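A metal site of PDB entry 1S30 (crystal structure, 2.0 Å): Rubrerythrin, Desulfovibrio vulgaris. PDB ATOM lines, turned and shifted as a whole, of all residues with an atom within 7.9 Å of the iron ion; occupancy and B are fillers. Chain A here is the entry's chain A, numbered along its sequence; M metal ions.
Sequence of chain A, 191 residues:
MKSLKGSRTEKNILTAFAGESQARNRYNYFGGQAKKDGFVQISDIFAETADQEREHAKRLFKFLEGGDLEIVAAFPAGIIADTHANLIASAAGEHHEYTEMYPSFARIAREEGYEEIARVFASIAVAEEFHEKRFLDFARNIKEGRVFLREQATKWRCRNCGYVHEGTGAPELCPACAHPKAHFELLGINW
The side-chain sulfur of Cys 161 sits close to the backbone NH of Tyr 163 (3.5 Å). The side-chain sulfur of Cys 174 sits close to the backbone NH of Ala 176 (3.4 Å). The backbone NH (N) of Cys 174 is in hydrogen-bond range of the backbone carbonyl oxygen (O) of His 179, at 2.8 Å. The side-chain amide oxygen (OD1) of Asn 160 lies close to the side-chain sulfur (SG) of Cys 177 (3.3 Å). O of Cys 177 is in hydrogen-bond range of ND1 of His 179. N of Cys 158 sits at hydrogen-bond distance from O of Tyr 163. The side-chain sulfur (SG) of Cys 158 lies close to the backbone NH (N) of Asn 160, 3.5 Å away.
Four residues have an atom within 4 Å of the iron ion: Cys 158, Cys 161, Cys 174 and Cys 177. The nearest printed residue that does not touch the iron ion is Tyr 163 (4.3 Å).
The side-chain sulfur (SG) of Cys 161 is bound to the iron ion, 2.2 Å away. SG of Cys 174 binds the iron ion, at 2.3 Å. The side-chain sulfur (SG) of Cys 177 is bound to the iron ion. SG of Cys 158 binds the iron ion, at 2.3 Å.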
ATOM      1  N   ARG A 157      -1.434   1.380   0.483  1.00  0.00           N
ATOM      2  CA  ARG A 157      -1.969   2.663   0.940  1.00  0.00           C
ATOM      3  C   ARG A 157      -3.037   2.478   2.013  1.00  0.00           C
ATOM      4  O   ARG A 157      -3.937   1.655   1.868  1.00  0.00           O
ATOM      5  CB  ARG A 157      -2.568   3.453  -0.243  1.00  0.00           C
ATOM      6  CG  ARG A 157      -3.000   4.879   0.148  1.00  0.00           C
ATOM      7  CD  ARG A 157      -3.813   5.588  -0.939  1.00  0.00           C
ATOM      8  NE  ARG A 157      -5.171   5.074  -1.059  1.00  0.00           N
ATOM      9  CZ  ARG A 157      -6.267   5.817  -0.950  1.00  0.00           C
ATOM     10  NH1 ARG A 157      -6.175   7.116  -0.713  1.00  0.00           N
ATOM     11  NH2 ARG A 157      -7.464   5.252  -1.068  1.00  0.00           N
ATOM     12  N   CYS A 158      -2.924   3.248   3.084  1.00  0.00           N
ATOM     13  CA  CYS A 158      -3.888   3.206   4.175  1.00  0.00           C
ATOM     14  C   CYS A 158      -5.089   4.036   3.716  1.00  0.00           C
ATOM     15  O   CYS A 158      -4.947   5.221   3.423  1.00  0.00           O
ATOM     16  CB  CYS A 158      -3.281   3.816   5.439  1.00  0.00           C
ATOM     17  SG  CYS A 158      -4.475   4.023   6.790  1.00  0.00           S
ATOM     18  N   ARG A 159      -6.259   3.416   3.679  1.00  0.00           N
ATOM     19  CA  ARG A 159      -7.463   4.117   3.245  1.00  0.00           C
ATOM     20  C   ARG A 159      -7.933   5.198   4.225  1.00  0.00           C
ATOM     21  O   ARG A 159      -8.601   6.143   3.841  1.00  0.00           O
ATOM     22  CB  ARG A 159      -8.601   3.129   3.003  1.00  0.00           C
ATOM     23  CG  ARG A 159      -8.433   2.270   1.754  1.00  0.00           C
ATOM     24  CD  ARG A 159      -9.616   1.316   1.588  1.00  0.00           C
ATOM     25  NE  ARG A 159     -10.877   2.031   1.373  1.00  0.00           N
ATOM     26  CZ  ARG A 159     -11.203   2.638   0.239  1.00  0.00           C
ATOM     27  NH1 ARG A 159     -10.363   2.633  -0.789  1.00  0.00           N
ATOM     28  NH2 ARG A 159     -12.355   3.283   0.128  1.00  0.00           N
ATOM     29  N   ASN A 160      -7.561   5.039   5.493  1.00  0.00           N
ATOM     30  CA  ASN A 160      -7.964   5.992   6.513  1.00  0.00           C
ATOM     31  C   ASN A 160      -7.214   7.326   6.492  1.00  0.00           C
ATOM     32  O   ASN A 160      -7.834   8.384   6.654  1.00  0.00           O
ATOM     33  CB  ASN A 160      -7.809   5.342   7.902  1.00  0.00           C
ATOM     34  CG  ASN A 160      -8.330   6.239   9.017  1.00  0.00           C
ATOM     35  OD1 ASN A 160      -7.563   6.686   9.873  1.00  0.00           O
ATOM     36  ND2 ASN A 160      -9.624   6.506   9.015  1.00  0.00           N
ATOM     37  N   CYS A 161      -5.907   7.297   6.269  1.00  0.00           N
ATOM     38  CA  CYS A 161      -5.105   8.526   6.271  1.00  0.00           C
ATOM     39  C   CYS A 161      -4.227   8.766   5.043  1.00  0.00           C
ATOM     40  O   CYS A 161      -3.644   9.834   4.904  1.00  0.00           O
ATOM     41  CB  CYS A 161      -4.205   8.555   7.513  1.00  0.00           C
ATOM     42  SG  CYS A 161      -2.776   7.447   7.433  1.00  0.00           S
ATOM     43  N   GLY A 162      -4.111   7.775   4.173  1.00  0.00           N
ATOM     44  CA  GLY A 162      -3.309   7.954   2.976  1.00  0.00           C
ATOM     45  C   GLY A 162      -1.834   7.596   3.077  1.00  0.00           C
ATOM     46  O   GLY A 162      -1.082   7.811   2.129  1.00  0.00           O
ATOM     47  N   TYR A 163      -1.395   7.082   4.222  1.00  0.00           N
ATOM     48  CA  TYR A 163       0.006   6.696   4.370  1.00  0.00           C
ATOM     49  C   TYR A 163       0.324   5.636   3.315  1.00  0.00           C
ATOM     50  O   TYR A 163      -0.502   4.781   3.012  1.00  0.00           O
ATOM     51  CB  TYR A 163       0.261   6.126   5.763  1.00  0.00           C
ATOM     52  CG  TYR A 163       1.674   5.609   5.970  1.00  0.00           C
ATOM     53  CD1 TYR A 163       2.757   6.484   6.132  1.00  0.00           C
ATOM     54  CD2 TYR A 163       1.943   4.239   5.946  1.00  0.00           C
ATOM     55  CE1 TYR A 163       4.059   6.009   6.266  1.00  0.00           C
ATOM     56  CE2 TYR A 163       3.251   3.759   6.075  1.00  0.00           C
ATOM     57  CZ  TYR A 163       4.294   4.645   6.234  1.00  0.00           C
ATOM     58  OH  TYR A 163       5.577   4.169   6.347  1.00  0.00           O
ATOM     59  N   VAL A 164       1.522   5.702   2.743  1.00  0.00           N
ATOM     60  CA  VAL A 164       1.937   4.724   1.752  1.00  0.00           C
ATOM     61  C   VAL A 164       3.041   3.865   2.363  1.00  0.00           C
ATOM     62  O   VAL A 164       4.013   4.381   2.905  1.00  0.00           O
ATOM     63  CB  VAL A 164       2.457   5.402   0.457  1.00  0.00           C
ATOM     64  CG1 VAL A 164       3.023   4.347  -0.495  1.00  0.00           C
ATOM     65  CG2 VAL A 164       1.327   6.159  -0.222  1.00  0.00           C
ATOM     66  N   LEU A 173      -0.063  -2.145  11.841  1.00  0.00           N
ATOM     67  CA  LEU A 173      -0.612  -0.861  12.264  1.00  0.00           C
ATOM     68  C   LEU A 173      -0.053   0.246  11.382  1.00  0.00           C
ATOM     69  O   LEU A 173       1.145   0.293  11.102  1.00  0.00           O
ATOM     70  CB  LEU A 173      -0.229  -0.562  13.715  1.00  0.00           C
ATOM     71  CG  LEU A 173      -0.849  -1.416  14.820  1.00  0.00           C
ATOM     72  CD1 LEU A 173      -0.245  -1.040  16.169  1.00  0.00           C
ATOM     73  CD2 LEU A 173      -2.355  -1.217  14.826  1.00  0.00           C
ATOM     74  N   CYS A 174      -0.930   1.146  10.929  1.00  0.00           N
ATOM     75  CA  CYS A 174      -0.463   2.249  10.109  1.00  0.00           C
ATOM     76  C   CYS A 174       0.381   3.144  11.016  1.00  0.00           C
ATOM     77  O   CYS A 174      -0.075   3.562  12.080  1.00  0.00           O
ATOM     78  CB  CYS A 174      -1.652   3.052   9.565  1.00  0.00           C
ATOM     79  SG  CYS A 174      -1.141   4.559   8.685  1.00  0.00           S
ATOM     80  N   PRO A 175       1.625   3.433  10.613  1.00  0.00           N
ATOM     81  CA  PRO A 175       2.479   4.282  11.446  1.00  0.00           C
ATOM     82  C   PRO A 175       2.056   5.746  11.546  1.00  0.00           C
ATOM     83  O   PRO A 175       2.541   6.482  12.396  1.00  0.00           O
ATOM     84  CB  PRO A 175       3.858   4.110  10.798  1.00  0.00           C
ATOM     85  CG  PRO A 175       3.518   3.925   9.362  1.00  0.00           C
ATOM     86  CD  PRO A 175       2.341   2.988   9.407  1.00  0.00           C
ATOM     87  N   ALA A 176       1.145   6.161  10.667  1.00  0.00           N
ATOM     88  CA  ALA A 176       0.673   7.539  10.680  1.00  0.00           C
ATOM     89  C   ALA A 176      -0.602   7.750  11.490  1.00  0.00           C
ATOM     90  O   ALA A 176      -0.679   8.655  12.310  1.00  0.00           O
ATOM     91  CB  ALA A 176       0.464   8.030   9.240  1.00  0.00           C
ATOM     92  N   CYS A 177      -1.602   6.893  11.283  1.00  0.00           N
ATOM     93  CA  CYS A 177      -2.872   7.040  12.006  1.00  0.00           C
ATOM     94  C   CYS A 177      -3.140   5.947  13.036  1.00  0.00           C
ATOM     95  O   CYS A 177      -4.161   5.977  13.723  1.00  0.00           O
ATOM     96  CB  CYS A 177      -4.035   7.105  11.010  1.00  0.00           C
ATOM     97  SG  CYS A 177      -4.437   5.540  10.208  1.00  0.00           S
ATOM     98  N   ALA A 178      -2.227   4.996  13.150  1.00  0.00           N
ATOM     99  CA  ALA A 178      -2.346   3.903  14.106  1.00  0.00           C
ATOM    100  C   ALA A 178      -3.544   2.980  13.905  1.00  0.00           C
ATOM    101  O   ALA A 178      -3.896   2.220  14.820  1.00  0.00           O
ATOM    102  CB  ALA A 178      -2.346   4.470  15.545  1.00  0.00           C
ATOM    103  N   HIS A 179      -4.188   3.032  12.747  1.00  0.00           N
ATOM    104  CA  HIS A 179      -5.307   2.124  12.514  1.00  0.00           C
ATOM    105  C   HIS A 179      -4.762   0.767  12.097  1.00  0.00           C
ATOM    106  O   HIS A 179      -3.640   0.686  11.606  1.00  0.00           O
ATOM    107  CB  HIS A 179      -6.245   2.681  11.437  1.00  0.00           C
ATOM    108  CG  HIS A 179      -7.219   3.686  11.959  1.00  0.00           C
ATOM    109  ND1 HIS A 179      -6.814   4.823  12.642  1.00  0.00           N
ATOM    110  CD2 HIS A 179      -8.574   3.723  11.942  1.00  0.00           C
ATOM    111  CE1 HIS A 179      -7.882   5.503  13.020  1.00  0.00           C
ATOM    112  NE2 HIS A 179      -8.963   4.862  12.605  1.00  0.00           N
ATOM    113  N   PRO A 180      -5.546  -0.304  12.300  1.00  0.00           N
ATOM    114  CA  PRO A 180      -5.115  -1.658  11.945  1.00  0.00           C
ATOM    115  C   PRO A 180      -4.927  -1.936  10.454  1.00  0.00           C
ATOM    116  O   PRO A 180      -5.404  -1.191   9.588  1.00  0.00           O
ATOM    117  CB  PRO A 180      -6.181  -2.533  12.577  1.00  0.00           C
ATOM    118  CG  PRO A 180      -7.399  -1.684  12.480  1.00  0.00           C
ATOM    119  CD  PRO A 180      -6.885  -0.318  12.890  1.00  0.00           C
ATOM    120  N   HIS A 183      -7.212  -1.527   7.111  1.00  0.00           N
ATOM    121  CA  HIS A 183      -7.433  -0.335   6.309  1.00  0.00           C
ATOM    122  C   HIS A 183      -6.557  -0.209   5.048  1.00  0.00           C
ATOM    123  O   HIS A 183      -6.772   0.689   4.231  1.00  0.00           O
ATOM    124  CB  HIS A 183      -7.251   0.911   7.193  1.00  0.00           C
ATOM    125  CG  HIS A 183      -8.312   1.059   8.240  1.00  0.00           C
ATOM    126  ND1 HIS A 183      -9.448   1.821   8.045  1.00  0.00           N
ATOM    127  CD2 HIS A 183      -8.433   0.509   9.463  1.00  0.00           C
ATOM    128  CE1 HIS A 183     -10.221   1.727   9.111  1.00  0.00           C
ATOM    129  NE2 HIS A 183      -9.629   0.939   9.989  1.00  0.00           N
ATOM    130  N   PHE A 184      -5.578  -1.093   4.886  1.00  0.00           N
ATOM    131  CA  PHE A 184      -4.689  -1.034   3.729  1.00  0.00           C
ATOM    132  C   PHE A 184      -5.176  -1.725   2.456  1.00  0.00           C
ATOM    133  O   PHE A 184      -5.916  -2.709   2.495  1.00  0.00           O
ATOM    134  CB  PHE A 184      -3.307  -1.575   4.096  1.00  0.00           C
ATOM    135  CG  PHE A 184      -2.516  -0.663   4.982  1.00  0.00           C
ATOM    136  CD1 PHE A 184      -2.668  -0.700   6.358  1.00  0.00           C
ATOM    137  CD2 PHE A 184      -1.632   0.259   4.424  1.00  0.00           C
ATOM    138  CE1 PHE A 184      -1.959   0.162   7.177  1.00  0.00           C
ATOM    139  CE2 PHE A 184      -0.913   1.132   5.234  1.00  0.00           C
ATOM    140  CZ  PHE A 184      -1.075   1.085   6.619  1.00  0.00           C
HETATM  141 FE    FE M   1      -3.237   5.402   8.230  1.00  0.00          FE
